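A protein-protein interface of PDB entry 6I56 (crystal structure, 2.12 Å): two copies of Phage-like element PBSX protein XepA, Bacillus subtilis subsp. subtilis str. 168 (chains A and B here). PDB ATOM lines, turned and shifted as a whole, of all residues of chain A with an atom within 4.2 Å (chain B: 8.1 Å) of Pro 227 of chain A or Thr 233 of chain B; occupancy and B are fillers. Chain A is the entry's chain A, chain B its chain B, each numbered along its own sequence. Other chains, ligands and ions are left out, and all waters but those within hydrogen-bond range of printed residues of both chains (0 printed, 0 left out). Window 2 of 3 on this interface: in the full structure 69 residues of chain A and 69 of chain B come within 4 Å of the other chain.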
ATOM      1  N   PHE A 216      32.060  22.865  12.905  1.00  0.00           N
ATOM      2  CA  PHE A 216      31.695  23.586  14.141  1.00  0.00           C
ATOM      3  C   PHE A 216      30.900  22.649  15.066  1.00  0.00           C
ATOM      4  O   PHE A 216      29.855  22.153  14.647  1.00  0.00           O
ATOM      5  CB  PHE A 216      30.897  24.845  13.801  1.00  0.00           C
ATOM      6  CG  PHE A 216      31.448  25.726  12.705  1.00  0.00           C
ATOM      7  CD1 PHE A 216      32.812  25.844  12.498  1.00  0.00           C
ATOM      8  CD2 PHE A 216      30.597  26.439  11.874  1.00  0.00           C
ATOM      9  CE1 PHE A 216      33.300  26.709  11.526  1.00  0.00           C
ATOM     10  CE2 PHE A 216      31.085  27.277  10.882  1.00  0.00           C
ATOM     11  CZ  PHE A 216      32.434  27.434  10.724  1.00  0.00           C
ATOM     12  N   TRP A 217      31.373  22.453  16.298  1.00  0.00           N
ATOM     13  CA  TRP A 217      30.792  21.534  17.298  1.00  0.00           C
ATOM     14  C   TRP A 217      30.591  22.199  18.661  1.00  0.00           C
ATOM     15  O   TRP A 217      31.438  22.980  19.074  1.00  0.00           O
ATOM     16  CB  TRP A 217      31.664  20.306  17.505  1.00  0.00           C
ATOM     17  CG  TRP A 217      31.978  19.429  16.331  1.00  0.00           C
ATOM     18  CD1 TRP A 217      33.210  19.278  15.767  1.00  0.00           C
ATOM     19  CD2 TRP A 217      31.125  18.474  15.696  1.00  0.00           C
ATOM     20  NE1 TRP A 217      33.181  18.311  14.809  1.00  0.00           N
ATOM     21  CE2 TRP A 217      31.921  17.793  14.746  1.00  0.00           C
ATOM     22  CE3 TRP A 217      29.780  18.115  15.839  1.00  0.00           C
ATOM     23  CZ2 TRP A 217      31.405  16.786  13.919  1.00  0.00           C
ATOM     24  CZ3 TRP A 217      29.261  17.120  15.025  1.00  0.00           C
ATOM     25  CH2 TRP A 217      30.077  16.442  14.102  1.00  0.00           C
ATOM     26  N   LEU A 226      27.778  17.992  18.977  1.00  0.00           N
ATOM     27  CA  LEU A 226      26.538  18.438  18.305  1.00  0.00           C
ATOM     28  C   LEU A 226      26.940  19.513  17.315  1.00  0.00           C
ATOM     29  O   LEU A 226      27.714  20.407  17.671  1.00  0.00           O
ATOM     30  CB  LEU A 226      25.573  18.980  19.354  1.00  0.00           C
ATOM     31  CG  LEU A 226      25.089  17.942  20.360  1.00  0.00           C
ATOM     32  CD1 LEU A 226      24.768  18.592  21.681  1.00  0.00           C
ATOM     33  CD2 LEU A 226      23.902  17.136  19.855  1.00  0.00           C
ATOM     34  N   PRO A 227      26.456  19.445  16.059  1.00  0.00           N
ATOM     35  CA  PRO A 227      26.798  20.463  15.075  1.00  0.00           C
ATOM     36  C   PRO A 227      26.129  21.774  15.505  1.00  0.00           C
ATOM     37  O   PRO A 227      24.945  21.777  15.928  1.00  0.00           O
ATOM     38  CB  PRO A 227      26.277  19.951  13.733  1.00  0.00           C
ATOM     39  CG  PRO A 227      25.619  18.581  14.033  1.00  0.00           C
ATOM     40  CD  PRO A 227      25.509  18.439  15.535  1.00  0.00           C
ATOM     41  N   ILE A 228      26.883  22.858  15.378  1.00  0.00           N
ATOM     42  CA  ILE A 228      26.376  24.223  15.682  1.00  0.00           C
ATOM     43  C   ILE A 228      26.585  25.090  14.458  1.00  0.00           C
ATOM     44  O   ILE A 228      27.488  24.771  13.653  1.00  0.00           O
ATOM     45  CB  ILE A 228      27.041  24.820  16.923  1.00  0.00           C
ATOM     46  CG1 ILE A 228      28.546  24.924  16.772  1.00  0.00           C
ATOM     47  CG2 ILE A 228      26.679  23.998  18.136  1.00  0.00           C
ATOM     48  CD1 ILE A 228      29.205  25.592  17.920  1.00  0.00           C
ATOM     49  N   ARG A 229      25.780  26.147  14.323  1.00  0.00           N
ATOM     50  CA  ARG A 229      25.817  27.031  13.134  1.00  0.00           C
ATOM     51  C   ARG A 229      26.437  28.368  13.525  1.00  0.00           C
ATOM     52  O   ARG A 229      26.095  28.905  14.578  1.00  0.00           O
ATOM     53  CB  ARG A 229      24.414  27.202  12.573  1.00  0.00           C
ATOM     54  CG  ARG A 229      23.968  25.959  11.824  1.00  0.00           C
ATOM     55  CD  ARG A 229      22.459  25.891  11.621  1.00  0.00           C
ATOM     56  NE  ARG A 229      21.750  26.917  10.860  1.00  0.00           N
ATOM     57  CZ  ARG A 229      21.737  26.982   9.534  1.00  0.00           C
ATOM     58  NH1 ARG A 229      22.526  26.186   8.851  1.00  0.00           N
ATOM     59  NH2 ARG A 229      21.039  27.907   8.913  1.00  0.00           N
ATOM     60  N   PHE A 256      25.934  25.704  26.171  1.00  0.00           N
ATOM     61  CA  PHE A 256      26.941  24.678  25.819  1.00  0.00           C
ATOM     62  C   PHE A 256      27.969  24.552  26.958  1.00  0.00           C
ATOM     63  O   PHE A 256      28.262  25.548  27.653  1.00  0.00           O
ATOM     64  CB  PHE A 256      27.589  24.990  24.472  1.00  0.00           C
ATOM     65  CG  PHE A 256      26.758  24.588  23.278  1.00  0.00           C
ATOM     66  CD1 PHE A 256      26.660  23.275  22.888  1.00  0.00           C
ATOM     67  CD2 PHE A 256      26.012  25.519  22.583  1.00  0.00           C
ATOM     68  CE1 PHE A 256      25.868  22.918  21.808  1.00  0.00           C
ATOM     69  CE2 PHE A 256      25.226  25.169  21.498  1.00  0.00           C
ATOM     70  CZ  PHE A 256      25.165  23.867  21.110  1.00  0.00           C
ATOM     71  N   HIS B 200      17.257  31.062  29.035  1.00  0.00           N
ATOM     72  CA  HIS B 200      17.626  30.239  27.857  1.00  0.00           C
ATOM     73  C   HIS B 200      17.892  28.796  28.290  1.00  0.00           C
ATOM     74  O   HIS B 200      18.456  28.578  29.376  1.00  0.00           O
ATOM     75  CB  HIS B 200      18.802  30.891  27.128  1.00  0.00           C
ATOM     76  CG  HIS B 200      19.019  30.344  25.761  1.00  0.00           C
ATOM     77  ND1 HIS B 200      19.907  29.274  25.517  1.00  0.00           N
ATOM     78  CD2 HIS B 200      18.449  30.666  24.567  1.00  0.00           C
ATOM     79  CE1 HIS B 200      19.905  29.008  24.218  1.00  0.00           C
ATOM     80  NE2 HIS B 200      19.015  29.862  23.620  1.00  0.00           N
ATOM     81  N   LEU B 201      17.463  27.838  27.474  1.00  0.00           N
ATOM     82  CA  LEU B 201      17.621  26.406  27.745  1.00  0.00           C
ATOM     83  C   LEU B 201      18.164  25.715  26.495  1.00  0.00           C
ATOM     84  O   LEU B 201      17.630  25.957  25.402  1.00  0.00           O
ATOM     85  CB  LEU B 201      16.275  25.833  28.187  1.00  0.00           C
ATOM     86  CG  LEU B 201      16.206  24.320  28.322  1.00  0.00           C
ATOM     87  CD1 LEU B 201      16.980  23.862  29.531  1.00  0.00           C
ATOM     88  CD2 LEU B 201      14.774  23.871  28.440  1.00  0.00           C
ATOM     89  N   LEU B 202      19.216  24.904  26.667  1.00  0.00           N
ATOM     90  CA  LEU B 202      19.702  23.978  25.620  1.00  0.00           C
ATOM     91  C   LEU B 202      19.374  22.552  26.053  1.00  0.00           C
ATOM     92  O   LEU B 202      19.773  22.163  27.138  1.00  0.00           O
ATOM     93  CB  LEU B 202      21.201  24.174  25.410  1.00  0.00           C
ATOM     94  CG  LEU B 202      21.805  23.303  24.308  1.00  0.00           C
ATOM     95  CD1 LEU B 202      21.316  23.725  22.928  1.00  0.00           C
ATOM     96  CD2 LEU B 202      23.322  23.329  24.366  1.00  0.00           C
ATOM     97  N   VAL B 203      18.643  21.822  25.217  1.00  0.00           N
ATOM     98  CA  VAL B 203      18.202  20.426  25.492  1.00  0.00           C
ATOM     99  C   VAL B 203      18.851  19.513  24.474  1.00  0.00           C
ATOM    100  O   VAL B 203      18.675  19.738  23.282  1.00  0.00           O
ATOM    101  CB  VAL B 203      16.668  20.273  25.459  1.00  0.00           C
ATOM    102  CG1 VAL B 203      16.276  18.835  25.744  1.00  0.00           C
ATOM    103  CG2 VAL B 203      15.997  21.204  26.452  1.00  0.00           C
ATOM    104  N   GLU B 204      19.541  18.501  24.969  1.00  0.00           N
ATOM    105  CA  GLU B 204      20.132  17.399  24.171  1.00  0.00           C
ATOM    106  C   GLU B 204      19.233  16.169  24.289  1.00  0.00           C
ATOM    107  O   GLU B 204      18.810  15.833  25.413  1.00  0.00           O
ATOM    108  CB  GLU B 204      21.539  17.087  24.680  1.00  0.00           C
ATOM    109  CG  GLU B 204      22.312  16.264  23.685  1.00  0.00           C
ATOM    110  CD  GLU B 204      23.650  15.745  24.173  1.00  0.00           C
ATOM    111  OE1 GLU B 204      23.943  15.934  25.414  1.00  0.00           O
ATOM    112  OE2 GLU B 204      24.360  15.141  23.295  1.00  0.00           O
ATOM    113  N   GLY B 230      11.371  25.120  19.921  1.00  0.00           N
ATOM    114  CA  GLY B 230      12.828  25.178  20.029  1.00  0.00           C
ATOM    115  C   GLY B 230      13.456  25.329  18.666  1.00  0.00           C
ATOM    116  O   GLY B 230      12.779  25.097  17.667  1.00  0.00           O
ATOM    117  N   VAL B 231      14.730  25.706  18.649  1.00  0.00           N
ATOM    118  CA  VAL B 231      15.514  25.882  17.402  1.00  0.00           C
ATOM    119  C   VAL B 231      16.646  24.838  17.446  1.00  0.00           C
ATOM    120  O   VAL B 231      17.467  24.826  18.406  1.00  0.00           O
ATOM    121  CB  VAL B 231      16.030  27.319  17.274  1.00  0.00           C
ATOM    122  CG1 VAL B 231      16.765  27.487  15.953  1.00  0.00           C
ATOM    123  CG2 VAL B 231      14.880  28.350  17.373  1.00  0.00           C
ATOM    124  N   LYS B 232      16.668  23.961  16.466  1.00  0.00           N
ATOM    125  CA  LYS B 232      17.658  22.864  16.418  1.00  0.00           C
ATOM    126  C   LYS B 232      19.019  23.455  16.020  1.00  0.00           C
ATOM    127  O   LYS B 232      19.063  24.266  15.098  1.00  0.00           O
ATOM    128  CB  LYS B 232      17.153  21.784  15.469  1.00  0.00           C
ATOM    129  CG  LYS B 232      18.046  20.565  15.412  1.00  0.00           C
ATOM    130  CD  LYS B 232      17.336  19.292  15.157  1.00  0.00           C
ATOM    131  CE  LYS B 232      16.787  19.224  13.777  1.00  0.00           C
ATOM    132  NZ  LYS B 232      17.894  18.894  12.831  1.00  0.00           N
ATOM    133  N   THR B 233      20.082  23.076  16.711  1.00  0.00           N
ATOM    134  CA  THR B 233      21.407  23.756  16.567  1.00  0.00           C
ATOM    135  C   THR B 233      21.993  23.567  15.162  1.00  0.00           C
ATOM    136  O   THR B 233      22.644  24.482  14.661  1.00  0.00           O
ATOM    137  CB  THR B 233      22.383  23.298  17.646  1.00  0.00           C
ATOM    138  OG1 THR B 233      22.754  21.930  17.414  1.00  0.00           O
ATOM    139  CG2 THR B 233      21.803  23.443  19.040  1.00  0.00           C
ATOM    140  N   ASP B 234      21.792  22.427  14.517  1.00  0.00           N
ATOM    141  CA  ASP B 234      22.543  22.099  13.271  1.00  0.00           C
ATOM    142  C   ASP B 234      21.921  22.800  12.065  1.00  0.00           C
ATOM    143  O   ASP B 234      22.712  23.166  11.226  1.00  0.00           O
ATOM    144  CB  ASP B 234      22.721  20.595  13.031  1.00  0.00           C
ATOM    145  CG  ASP B 234      21.453  19.782  12.886  1.00  0.00           C
ATOM    146  OD1 ASP B 234      20.318  20.392  12.920  1.00  0.00           O
ATOM    147  OD2 ASP B 234      21.610  18.565  12.721  1.00  0.00           O
ATOM    148  N   ASP B 235      20.604  23.012  11.992  1.00  0.00           N
ATOM    149  CA  ASP B 235      19.940  23.526  10.765  1.00  0.00           C
ATOM    150  C   ASP B 235      18.892  24.610  11.084  1.00  0.00           C
ATOM    151  O   ASP B 235      18.292  25.098  10.150  1.00  0.00           O
ATOM    152  CB  ASP B 235      19.331  22.372   9.960  1.00  0.00           C
ATOM    153  CG  ASP B 235      18.252  21.623  10.706  1.00  0.00           C
ATOM    154  OD1 ASP B 235      17.822  22.082  11.789  1.00  0.00           O
ATOM    155  OD2 ASP B 235      17.898  20.553  10.244  1.00  0.00           O
ATOM    156  N   ALA B 236      18.677  24.990  12.342  1.00  0.00           N
ATOM    157  CA  ALA B 236      17.784  26.114  12.700  1.00  0.00           C
ATOM    158  C   ALA B 236      16.317  25.745  12.415  1.00  0.00           C
ATOM    159  O   ALA B 236      15.512  26.617  12.337  1.00  0.00           O
ATOM    160  CB  ALA B 236      18.185  27.373  11.971  1.00  0.00           C
ATOM    161  N   THR B 237      15.990  24.466  12.327  1.00  0.00           N
ATOM    162  CA  THR B 237      14.607  23.977  12.375  1.00  0.00           C
ATOM    163  C   THR B 237      13.938  24.514  13.644  1.00  0.00           C
ATOM    164  O   THR B 237      14.495  24.318  14.730  1.00  0.00           O
ATOM    165  CB  THR B 237      14.558  22.449  12.378  1.00  0.00           C
ATOM    166  OG1 THR B 237      15.218  22.013  11.205  1.00  0.00           O
ATOM    167  CG2 THR B 237      13.131  21.919  12.409  1.00  0.00           C
ATOM    168  N   ALA B 246      20.293  12.432  18.858  1.00  0.00           N
ATOM    169  CA  ALA B 246      21.658  12.962  18.600  1.00  0.00           C
ATOM    170  C   ALA B 246      21.486  14.375  18.054  1.00  0.00           C
ATOM    171  O   ALA B 246      22.027  14.674  17.010  1.00  0.00           O
ATOM    172  CB  ALA B 246      22.425  12.051  17.666  1.00  0.00           C
ATOM    173  N   GLU B 247      20.700  15.188  18.745  1.00  0.00           N
ATOM    174  CA  GLU B 247      20.394  16.588  18.328  1.00  0.00           C
ATOM    175  C   GLU B 247      20.151  17.433  19.578  1.00  0.00           C
ATOM    176  O   GLU B 247      20.009  16.878  20.709  1.00  0.00           O
ATOM    177  CB  GLU B 247      19.226  16.616  17.336  1.00  0.00           C
ATOM    178  CG  GLU B 247      17.965  15.957  17.864  1.00  0.00           C
ATOM    179  CD  GLU B 247      16.731  15.975  16.968  1.00  0.00           C
ATOM    180  OE1 GLU B 247      16.864  15.752  15.745  1.00  0.00           O
ATOM    181  OE2 GLU B 247      15.628  16.154  17.531  1.00  0.00           O
ATOM    182  N   ALA B 248      20.189  18.744  19.399  1.00  0.00           N
ATOM    183  CA  ALA B 248      19.997  19.700  20.503  1.00  0.00           C
ATOM    184  C   ALA B 248      19.090  20.828  20.042  1.00  0.00           C
ATOM    185  O   ALA B 248      19.187  21.273  18.879  1.00  0.00           O
ATOM    186  CB  ALA B 248      21.339  20.195  20.979  1.00  0.00           C
ATOM    187  N   TRP B 249      18.291  21.303  20.972  1.00  0.00           N
ATOM    188  CA  TRP B 249      17.247  22.327  20.746  1.00  0.00           C
ATOM    189  C   TRP B 249      17.445  23.464  21.754  1.00  0.00           C
ATOM    190  O   TRP B 249      17.583  23.163  22.977  1.00  0.00           O
ATOM    191  CB  TRP B 249      15.885  21.663  20.902  1.00  0.00           C
ATOM    192  CG  TRP B 249      15.603  20.613  19.880  1.00  0.00           C
ATOM    193  CD1 TRP B 249      15.966  19.305  19.935  1.00  0.00           C
ATOM    194  CD2 TRP B 249      14.894  20.789  18.647  1.00  0.00           C
ATOM    195  NE1 TRP B 249      15.545  18.656  18.810  1.00  0.00           N
ATOM    196  CE2 TRP B 249      14.887  19.539  17.998  1.00  0.00           C
ATOM    197  CE3 TRP B 249      14.243  21.874  18.046  1.00  0.00           C
ATOM    198  CZ2 TRP B 249      14.293  19.351  16.755  1.00  0.00           C
ATOM    199  CZ3 TRP B 249      13.619  21.678  16.837  1.00  0.00           C
ATOM    200  CH2 TRP B 249      13.655  20.436  16.194  1.00  0.00           C
ATOM    201  N   ALA B 250      17.417  24.700  21.256  1.00  0.00           N
ATOM    202  CA  ALA B 250      17.547  25.936  22.058  1.00  0.00           C
ATOM    203  C   ALA B 250      16.155  26.547  22.235  1.00  0.00           C
ATOM    204  O   ALA B 250      15.428  26.648  21.237  1.00  0.00           O
ATOM    205  CB  ALA B 250      18.498  26.900  21.401  1.00  0.00           C
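Hydrophobic or aromatic side chains of chain A within 4 Å of the printed part of chain B: Leu 226, Pro 227 and Phe 256.
Of the 18 printed residues of chain B, 8 touch a printed residue of chain A.
Hydrophobic or aromatic side chains of chain B within 4 Å of the printed part of chain A: Leu 202, Ala 236 and Ala 248.
Among the printed residues, 12 pairs touch across the chains.
Among the printed residues, no Asp or Glu carboxylate lies within 4 Å of a Lys or Arg side-chain nitrogen of the other chain.
Glu 204 of chain B touches Leu 226 of chain A (OE2 to CD1, 3.8 Å).
C of Glu 247 of chain B touches CD2 of Leu 226 of chain A, 3.8 Å away.
Ala 248 of chain B touches Leu 226 of chain A.
Asp 234 of chain B touches Pro 227 of chain A (N to O, 3.5 Å).
Ile 228 of chain A touches Thr 233 of chain B (CA to O, 3.9 Å).
CD of Arg 229 of chain A touches O of Asp 234 of chain B, at 2.8 Å.
Arg 229 of chain A touches Asp 235 of chain B (CD to N, 3.4 Å).
Arg 229 of chain A touches Ala 236 of chain B (NE to CB, 3.8 Å).
Leu 202 of chain B touches Phe 256 of chain A (CD2 to CE1, 3.6 Å).
CZ of Phe 256 of chain A touches CG2 of Thr 233 of chain B, at 3.97 Å.
Of chain B, only Thr 233 (2.7 Å) and Asp 234 (3.5 Å) come within 4 Å of Pro 227 of chain A.
Of the printed residues of chain A, Thr 233 of chain B touches Pro 227 (2.7 Å), Ile 228 (3.9 Å), Arg 229 (3.4 Å) and Phe 256 (3.97 Å).
Of the printed residues of chain A, Asp 234 of chain B touches Pro 227 and Arg 229.
Of the printed residues of chain A, Leu 202 of chain B touches Phe 256.
Leu 201 of chain B touches none of the printed residues of chain A.
The nearest residue of chain B that does not touch Pro 227 of chain A is Ala 246 of chain B (5.3 Å).
The nearest printed residue of chain A that does not touch Asp 235 of chain B is Pro 227 of chain A (6.0 Å).
No position is printed for both chains.
Of the 12 pairs that touch across the chains among the printed residues, none has its exchanged pair printed and touching as well.
The backbone carbonyl oxygen (O) of Phe 216 of chain A is in hydrogen-bond range of the backbone NH (N) of Ile 228 of chain A, 3.1 Å away.
The side-chain amino group (NZ) of Lys 232 of chain B is in salt-bridge range of the side-chain carboxylate (OD1) of Asp 234 of chain B (2.9 Å).
NZ of Lys 232 of chain B is in salt-bridge range of OD2 of Asp 235 of chain B (3.1 Å).
The backbone NH of Thr 233 of chain B lies within hydrogen-bond range of the backbone carbonyl oxygen of Ala 248 of chain B, at 3.0 Å.
OD1 of Asp 235 of chain B sits at hydrogen-bond distance from OG1 of Thr 237 of chain B, at 2.7 Å.
The side-chain carboxylate (OE2) of Glu 247 of chain B is in hydrogen-bond range of the indole nitrogen (NE1) of Trp 249 of chain B, at 2.8 Å.
O of Pro 227 of chain A sits at hydrogen-bond distance from OG1 of Thr 233 of chain B, 2.7 Å away.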
